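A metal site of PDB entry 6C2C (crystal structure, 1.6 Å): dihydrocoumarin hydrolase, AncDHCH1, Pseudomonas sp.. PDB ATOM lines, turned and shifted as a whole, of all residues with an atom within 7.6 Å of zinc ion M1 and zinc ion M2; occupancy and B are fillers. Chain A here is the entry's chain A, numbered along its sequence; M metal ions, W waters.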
ATOM      1  N   SER A  68      -0.870  -2.799  27.221  1.00  0.00           N
ATOM      2  CA  SER A  68      -2.011  -3.033  28.089  1.00  0.00           C
ATOM      3  C   SER A  68      -3.157  -3.683  27.351  1.00  0.00           C
ATOM      4  O   SER A  68      -3.328  -3.486  26.157  1.00  0.00           O
ATOM      5  CB  SER A  68      -2.509  -1.726  28.654  1.00  0.00           C
ATOM      6  OG  SER A  68      -1.594  -1.249  29.635  1.00  0.00           O
ATOM      7  N   VAL A  69      -3.953  -4.429  28.105  1.00  0.00           N
ATOM      8  CA  VAL A  69      -5.200  -5.014  27.644  1.00  0.00           C
ATOM      9  C   VAL A  69      -6.260  -4.601  28.640  1.00  0.00           C
ATOM     10  O   VAL A  69      -6.258  -5.090  29.786  1.00  0.00           O
ATOM     11  CB  VAL A  69      -5.132  -6.551  27.528  1.00  0.00           C
ATOM     12  CG1 VAL A  69      -6.545  -7.163  27.060  1.00  0.00           C
ATOM     13  CG2 VAL A  69      -4.047  -6.997  26.514  1.00  0.00           C
ATOM     14  N   ASN A  70      -7.185  -3.747  28.222  1.00  0.00           N
ATOM     15  CA  ASN A  70      -8.154  -3.122  29.145  1.00  0.00           C
ATOM     16  C   ASN A  70      -9.580  -3.494  28.798  1.00  0.00           C
ATOM     17  O   ASN A  70      -9.911  -3.763  27.634  1.00  0.00           O
ATOM     18  CB  ASN A  70      -8.068  -1.610  29.077  1.00  0.00           C
ATOM     19  CG  ASN A  70      -6.625  -1.059  29.193  1.00  0.00           C
ATOM     20  OD1 ASN A  70      -5.788  -1.579  29.956  1.00  0.00           O
ATOM     21  ND2 ASN A  70      -6.345   0.016  28.452  1.00  0.00           N
ATOM     22  N   ASP A  84     -15.906  -5.471  27.090  1.00  0.00           N
ATOM     23  CA  ASP A  84     -14.790  -6.380  26.882  1.00  0.00           C
ATOM     24  C   ASP A  84     -14.436  -7.180  28.146  1.00  0.00           C
ATOM     25  O   ASP A  84     -14.883  -6.827  29.177  1.00  0.00           O
ATOM     26  CB  ASP A  84     -13.615  -5.726  26.248  1.00  0.00           C
ATOM     27  CG  ASP A  84     -13.862  -5.409  24.758  1.00  0.00           C
ATOM     28  OD1 ASP A  84     -14.812  -5.961  24.192  1.00  0.00           O
ATOM     29  OD2 ASP A  84     -13.091  -4.620  24.242  1.00  0.00           O
ATOM     30  N   THR A 118     -16.323  -5.423  21.939  1.00  0.00           N
ATOM     31  CA  THR A 118     -15.977  -4.557  20.809  1.00  0.00           C
ATOM     32  C   THR A 118     -15.678  -5.383  19.554  1.00  0.00           C
ATOM     33  O   THR A 118     -16.102  -5.023  18.466  1.00  0.00           O
ATOM     34  CB  THR A 118     -14.756  -3.667  21.161  1.00  0.00           C
ATOM     35  OG1 THR A 118     -13.618  -4.497  21.498  1.00  0.00           O
ATOM     36  CG2 THR A 118     -15.096  -2.682  22.291  1.00  0.00           C
ATOM     37  N   HIS A 119     -15.036  -6.529  19.740  1.00  0.00           N
ATOM     38  CA  HIS A 119     -14.747  -7.447  18.646  1.00  0.00           C
ATOM     39  C   HIS A 119     -14.271  -8.763  19.244  1.00  0.00           C
ATOM     40  O   HIS A 119     -13.830  -8.812  20.393  1.00  0.00           O
ATOM     41  CB  HIS A 119     -13.692  -6.871  17.692  1.00  0.00           C
ATOM     42  CG  HIS A 119     -12.327  -6.659  18.286  1.00  0.00           C
ATOM     43  ND1 HIS A 119     -12.078  -5.819  19.362  1.00  0.00           N
ATOM     44  CD2 HIS A 119     -11.116  -7.150  17.903  1.00  0.00           C
ATOM     45  CE1 HIS A 119     -10.778  -5.817  19.627  1.00  0.00           C
ATOM     46  NE2 HIS A 119     -10.151  -6.585  18.735  1.00  0.00           N
ATOM     47  N   MET A 120     -14.390  -9.837  18.444  1.00  0.00           N
ATOM     48  CA  MET A 120     -14.135 -11.172  19.028  1.00  0.00           C
ATOM     49  C   MET A 120     -12.703 -11.657  18.919  1.00  0.00           C
ATOM     50  O   MET A 120     -12.470 -12.854  18.834  1.00  0.00           O
ATOM     51  CB  MET A 120     -15.096 -12.187  18.415  1.00  0.00           C
ATOM     52  CG  MET A 120     -16.556 -11.805  18.769  1.00  0.00           C
ATOM     53  SD  MET A 120     -17.696 -13.110  18.191  1.00  0.00           S
ATOM     54  CE  MET A 120     -19.231 -12.341  18.742  1.00  0.00           C
ATOM     55  N   HIS A 121     -11.713 -10.800  19.069  1.00  0.00           N
ATOM     56  CA  HIS A 121     -10.359 -11.256  19.255  1.00  0.00           C
ATOM     57  C   HIS A 121     -10.184 -11.851  20.639  1.00  0.00           C
ATOM     58  O   HIS A 121     -10.958 -11.568  21.566  1.00  0.00           O
ATOM     59  CB  HIS A 121      -9.391 -10.084  19.028  1.00  0.00           C
ATOM     60  CG  HIS A 121      -9.135  -9.788  17.582  1.00  0.00           C
ATOM     61  ND1 HIS A 121      -8.517  -8.657  17.122  1.00  0.00           N
ATOM     62  CD2 HIS A 121      -9.438 -10.505  16.460  1.00  0.00           C
ATOM     63  CE1 HIS A 121      -8.419  -8.658  15.801  1.00  0.00           C
ATOM     64  NE2 HIS A 121      -8.968  -9.785  15.376  1.00  0.00           N
ATOM     65  N   PRO A 122      -9.192 -12.718  20.809  1.00  0.00           N
ATOM     66  CA  PRO A 122      -9.103 -13.503  22.041  1.00  0.00           C
ATOM     67  C   PRO A 122      -8.924 -12.685  23.282  1.00  0.00           C
ATOM     68  O   PRO A 122      -9.416 -13.084  24.324  1.00  0.00           O
ATOM     69  CB  PRO A 122      -7.867 -14.386  21.817  1.00  0.00           C
ATOM     70  CG  PRO A 122      -7.117 -13.683  20.785  1.00  0.00           C
ATOM     71  CD  PRO A 122      -8.167 -13.126  19.842  1.00  0.00           C
ATOM     72  N   ASP A 123      -8.247 -11.557  23.181  1.00  0.00           N
ATOM     73  CA  ASP A 123      -7.985 -10.683  24.319  1.00  0.00           C
ATOM     74  C   ASP A 123      -9.165  -9.800  24.623  1.00  0.00           C
ATOM     75  O   ASP A 123      -9.078  -8.982  25.539  1.00  0.00           O
ATOM     76  CB  ASP A 123      -6.751  -9.816  24.061  1.00  0.00           C
ATOM     77  CG  ASP A 123      -6.818  -9.011  22.703  1.00  0.00           C
ATOM     78  OD1 ASP A 123      -7.181  -9.492  21.630  1.00  0.00           O
ATOM     79  OD2 ASP A 123      -6.480  -7.864  22.757  1.00  0.00           O
ATOM     80  N   HIS A 124     -10.308 -10.030  23.976  1.00  0.00           N
ATOM     81  CA  HIS A 124     -11.542  -9.342  24.362  1.00  0.00           C
ATOM     82  C   HIS A 124     -12.669 -10.271  24.774  1.00  0.00           C
ATOM     83  O   HIS A 124     -13.516  -9.874  25.599  1.00  0.00           O
ATOM     84  CB  HIS A 124     -12.033  -8.438  23.220  1.00  0.00           C
ATOM     85  CG  HIS A 124     -10.940  -7.449  22.833  1.00  0.00           C
ATOM     86  ND1 HIS A 124     -10.930  -6.128  23.237  1.00  0.00           N
ATOM     87  CD2 HIS A 124      -9.770  -7.661  22.171  1.00  0.00           C
ATOM     88  CE1 HIS A 124      -9.802  -5.564  22.831  1.00  0.00           C
ATOM     89  NE2 HIS A 124      -9.074  -6.488  22.192  1.00  0.00           N
ATOM     90  N   PHE A 167      -7.741 -17.929  16.698  1.00  0.00           N
ATOM     91  CA  PHE A 167      -8.650 -16.819  16.937  1.00  0.00           C
ATOM     92  C   PHE A 167     -10.100 -17.295  16.850  1.00  0.00           C
ATOM     93  O   PHE A 167     -10.952 -16.930  17.679  1.00  0.00           O
ATOM     94  CB  PHE A 167      -8.424 -15.685  15.934  1.00  0.00           C
ATOM     95  CG  PHE A 167      -7.190 -14.892  16.195  1.00  0.00           C
ATOM     96  CD1 PHE A 167      -6.130 -15.447  16.916  1.00  0.00           C
ATOM     97  CD2 PHE A 167      -7.101 -13.582  15.727  1.00  0.00           C
ATOM     98  CE1 PHE A 167      -4.982 -14.711  17.178  1.00  0.00           C
ATOM     99  CE2 PHE A 167      -5.939 -12.831  15.975  1.00  0.00           C
ATOM    100  CZ  PHE A 167      -4.885 -13.410  16.694  1.00  0.00           C
ATOM    101  N   HIS A 205     -11.121  -3.146  11.885  1.00  0.00           N
ATOM    102  CA  HIS A 205     -10.200  -3.989  12.647  1.00  0.00           C
ATOM    103  C   HIS A 205     -10.669  -5.468  12.613  1.00  0.00           C
ATOM    104  O   HIS A 205      -9.897  -6.357  12.543  1.00  0.00           O
ATOM    105  CB  HIS A 205     -10.065  -3.474  14.062  1.00  0.00           C
ATOM    106  CG  HIS A 205      -9.163  -4.281  14.907  1.00  0.00           C
ATOM    107  ND1 HIS A 205      -7.818  -4.392  14.667  1.00  0.00           N
ATOM    108  CD2 HIS A 205      -9.409  -5.023  15.992  1.00  0.00           C
ATOM    109  CE1 HIS A 205      -7.288  -5.172  15.582  1.00  0.00           C
ATOM    110  NE2 HIS A 205      -8.233  -5.572  16.379  1.00  0.00           N
ATOM    111  N   THR A 206     -11.988  -5.601  12.727  1.00  0.00           N
ATOM    112  CA  THR A 206     -12.683  -6.842  12.404  1.00  0.00           C
ATOM    113  C   THR A 206     -13.961  -6.457  11.667  1.00  0.00           C
ATOM    114  O   THR A 206     -14.400  -5.315  11.777  1.00  0.00           O
ATOM    115  CB  THR A 206     -13.014  -7.657  13.664  1.00  0.00           C
ATOM    116  OG1 THR A 206     -14.000  -6.944  14.440  1.00  0.00           O
ATOM    117  CG2 THR A 206     -11.763  -7.963  14.481  1.00  0.00           C
ATOM    118  N   HIS A 209     -16.298  -4.778  14.211  1.00  0.00           N
ATOM    119  CA  HIS A 209     -15.722  -4.034  15.320  1.00  0.00           C
ATOM    120  C   HIS A 209     -16.648  -2.866  15.681  1.00  0.00           C
ATOM    121  O   HIS A 209     -17.136  -2.143  14.807  1.00  0.00           O
ATOM    122  CB  HIS A 209     -14.311  -3.536  14.958  1.00  0.00           C
ATOM    123  CG  HIS A 209     -13.632  -2.837  16.109  1.00  0.00           C
ATOM    124  ND1 HIS A 209     -13.946  -1.528  16.453  1.00  0.00           N
ATOM    125  CD2 HIS A 209     -12.729  -3.273  17.021  1.00  0.00           C
ATOM    126  CE1 HIS A 209     -13.223  -1.202  17.534  1.00  0.00           C
ATOM    127  NE2 HIS A 209     -12.483  -2.234  17.881  1.00  0.00           N
ATOM    128  N   GLY A 225     -12.392   0.278  21.707  1.00  0.00           N
ATOM    129  CA  GLY A 225     -11.944  -1.089  21.363  1.00  0.00           C
ATOM    130  C   GLY A 225     -10.515  -1.041  20.875  1.00  0.00           C
ATOM    131  O   GLY A 225      -9.638  -0.454  21.523  1.00  0.00           O
ATOM    132  N   ASP A 226     -10.298  -1.626  19.719  1.00  0.00           N
ATOM    133  CA  ASP A 226      -8.997  -1.647  19.091  1.00  0.00           C
ATOM    134  C   ASP A 226      -8.774  -0.707  17.869  1.00  0.00           C
ATOM    135  O   ASP A 226      -8.182  -1.074  16.895  1.00  0.00           O
ATOM    136  CB  ASP A 226      -8.650  -3.081  18.708  1.00  0.00           C
ATOM    137  CG  ASP A 226      -8.247  -3.953  19.887  1.00  0.00           C
ATOM    138  OD1 ASP A 226      -8.419  -3.603  20.973  1.00  0.00           O
ATOM    139  OD2 ASP A 226      -7.818  -5.006  19.609  1.00  0.00           O
ATOM    140  N   LEU A 227      -9.375   0.455  17.934  1.00  0.00           N
ATOM    141  CA  LEU A 227      -9.044   1.471  16.926  1.00  0.00           C
ATOM    142  C   LEU A 227      -7.598   1.934  17.030  1.00  0.00           C
ATOM    143  O   LEU A 227      -7.130   2.625  16.137  1.00  0.00           O
ATOM    144  CB  LEU A 227      -9.974   2.684  17.020  1.00  0.00           C
ATOM    145  CG  LEU A 227     -11.461   2.502  16.723  1.00  0.00           C
ATOM    146  CD1 LEU A 227     -12.204   3.822  16.500  1.00  0.00           C
ATOM    147  CD2 LEU A 227     -11.761   1.492  15.591  1.00  0.00           C
ATOM    148  N   ILE A 228      -6.866   1.590  18.105  1.00  0.00           N
ATOM    149  CA  ILE A 228      -5.459   1.945  18.200  1.00  0.00           C
ATOM    150  C   ILE A 228      -4.729   0.811  18.915  1.00  0.00           C
ATOM    151  O   ILE A 228      -5.301   0.140  19.781  1.00  0.00           O
ATOM    152  CB  ILE A 228      -5.285   3.312  18.888  1.00  0.00           C
ATOM    153  CG1 ILE A 228      -3.800   3.751  18.989  1.00  0.00           C
ATOM    154  CG2 ILE A 228      -5.874   3.253  20.267  1.00  0.00           C
ATOM    155  CD1 ILE A 228      -3.610   5.305  18.912  1.00  0.00           C
ATOM    156  N   HIS A 229      -3.465   0.544  18.520  1.00  0.00           N
ATOM    157  CA  HIS A 229      -2.634  -0.418  19.215  1.00  0.00           C
ATOM    158  C   HIS A 229      -1.357   0.163  19.770  1.00  0.00           C
ATOM    159  O   HIS A 229      -0.829  -0.383  20.753  1.00  0.00           O
ATOM    160  CB  HIS A 229      -2.225  -1.605  18.334  1.00  0.00           C
ATOM    161  CG  HIS A 229      -3.375  -2.508  18.002  1.00  0.00           C
ATOM    162  ND1 HIS A 229      -4.343  -2.150  17.074  1.00  0.00           N
ATOM    163  CD2 HIS A 229      -3.721  -3.719  18.483  1.00  0.00           C
ATOM    164  CE1 HIS A 229      -5.225  -3.126  16.997  1.00  0.00           C
ATOM    165  NE2 HIS A 229      -4.864  -4.102  17.810  1.00  0.00           N
ATOM    166  N   ILE A 242      -2.021  -2.127  11.345  1.00  0.00           N
ATOM    167  CA  ILE A 242      -1.356  -3.252  11.996  1.00  0.00           C
ATOM    168  C   ILE A 242      -1.857  -4.555  11.380  1.00  0.00           C
ATOM    169  O   ILE A 242      -2.984  -4.634  10.858  1.00  0.00           O
ATOM    170  CB  ILE A 242      -1.578  -3.181  13.541  1.00  0.00           C
ATOM    171  CG1 ILE A 242      -0.627  -4.095  14.321  1.00  0.00           C
ATOM    172  CG2 ILE A 242      -3.073  -3.464  13.939  1.00  0.00           C
ATOM    173  CD1 ILE A 242      -0.547  -3.622  15.845  1.00  0.00           C
ATOM    174  N   PHE A 244      -2.944  -7.101  12.752  1.00  0.00           N
ATOM    175  CA  PHE A 244      -4.135  -7.639  13.388  1.00  0.00           C
ATOM    176  C   PHE A 244      -5.434  -7.150  12.733  1.00  0.00           C
ATOM    177  O   PHE A 244      -6.485  -7.691  13.039  1.00  0.00           O
ATOM    178  CB  PHE A 244      -4.174  -7.248  14.871  1.00  0.00           C
ATOM    179  CG  PHE A 244      -3.002  -7.720  15.678  1.00  0.00           C
ATOM    180  CD1 PHE A 244      -2.505  -9.009  15.530  1.00  0.00           C
ATOM    181  CD2 PHE A 244      -2.412  -6.850  16.623  1.00  0.00           C
ATOM    182  CE1 PHE A 244      -1.451  -9.442  16.305  1.00  0.00           C
ATOM    183  CE2 PHE A 244      -1.353  -7.288  17.390  1.00  0.00           C
ATOM    184  CZ  PHE A 244      -0.897  -8.590  17.240  1.00  0.00           C
ATOM    185  N   ASP A 245      -5.403  -6.095  11.938  1.00  0.00           N
ATOM    186  CA  ASP A 245      -6.612  -5.588  11.293  1.00  0.00           C
ATOM    187  C   ASP A 245      -7.102  -6.559  10.231  1.00  0.00           C
ATOM    188  O   ASP A 245      -6.314  -6.957   9.363  1.00  0.00           O
ATOM    189  CB  ASP A 245      -6.357  -4.244  10.602  1.00  0.00           C
ATOM    190  CG  ASP A 245      -6.033  -3.125  11.583  1.00  0.00           C
ATOM    191  OD1 ASP A 245      -6.590  -3.068  12.699  1.00  0.00           O
ATOM    192  OD2 ASP A 245      -5.225  -2.248  11.201  1.00  0.00           O
ATOM    193  N   ALA A 272      -8.732  -0.188  24.507  1.00  0.00           N
ATOM    194  CA  ALA A 272      -8.263  -1.477  25.050  1.00  0.00           C
ATOM    195  C   ALA A 272      -6.740  -1.596  25.120  1.00  0.00           C
ATOM    196  O   ALA A 272      -6.237  -2.290  26.023  1.00  0.00           O
ATOM    197  CB  ALA A 272      -8.784  -2.638  24.179  1.00  0.00           C
ATOM    198  N   HIS A 273      -5.990  -0.894  24.227  1.00  0.00           N
ATOM    199  CA  HIS A 273      -4.528  -1.080  24.179  1.00  0.00           C
ATOM    200  C   HIS A 273      -3.778   0.229  24.378  1.00  0.00           C
ATOM    201  O   HIS A 273      -2.590   0.304  24.040  1.00  0.00           O
ATOM    202  CB  HIS A 273      -4.099  -1.782  22.858  1.00  0.00           C
ATOM    203  CG  HIS A 273      -4.735  -3.158  22.742  1.00  0.00           C
ATOM    204  ND1 HIS A 273      -4.714  -4.078  23.777  1.00  0.00           N
ATOM    205  CD2 HIS A 273      -5.459  -3.704  21.760  1.00  0.00           C
ATOM    206  CE1 HIS A 273      -5.394  -5.160  23.410  1.00  0.00           C
ATOM    207  NE2 HIS A 273      -5.857  -4.960  22.202  1.00  0.00           N
HETATM  208 ZN    ZN M   1      -8.062  -6.788  18.351  1.00  0.00          ZN
HETATM  209 ZN    ZN M   2      -7.228  -6.309  21.203  1.00  0.00          ZN
HETATM  210  O   HOH W   1      -5.948  -6.727  17.642  1.00  0.00           O
HETATM  211  O   HOH W   2      -7.300  -7.604  19.871  1.00  0.00           O
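A ring nitrogen (ND1) of His 124 is in hydrogen-bond range of the side-chain carboxylate (OD2) of Asp 84. OG1 of Thr 118 lies within hydrogen-bond range of ND1 of His 119 (2.9 Å). NE2 of His 209 is in hydrogen-bond range of N of Asp 226 (2.9 Å). O of Ser 68 sits at hydrogen-bond distance from ND1 of His 273 (2.8 Å). ND1 of His 205 is in hydrogen-bond range of OD1 of Asp 245.
Of the 25 residues printed, 5 come within 4 Å of zinc ion M1. The nearest printed residue that does not touch zinc ion M1 is His 229 (4.2 Å).
Zinc ion M1 is bound by water W2 (1.9 Å), NE2 of His 119 (2.1 Å), OD2 of Asp 226 (2.2 Å), water W1 (2.2 Å), ND1 of His 121 (2.3 Å) and NE2 of His 205 (2.3 Å). Zinc ion M1 has six donor atoms within binding distance.
Zinc ion M2 is bound by water W2, NE2 of His 124, OD2 of Asp 226, NE2 of His 273 and OD2 of Asp 123. Zinc ion M2 has five donor atoms within binding distance.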
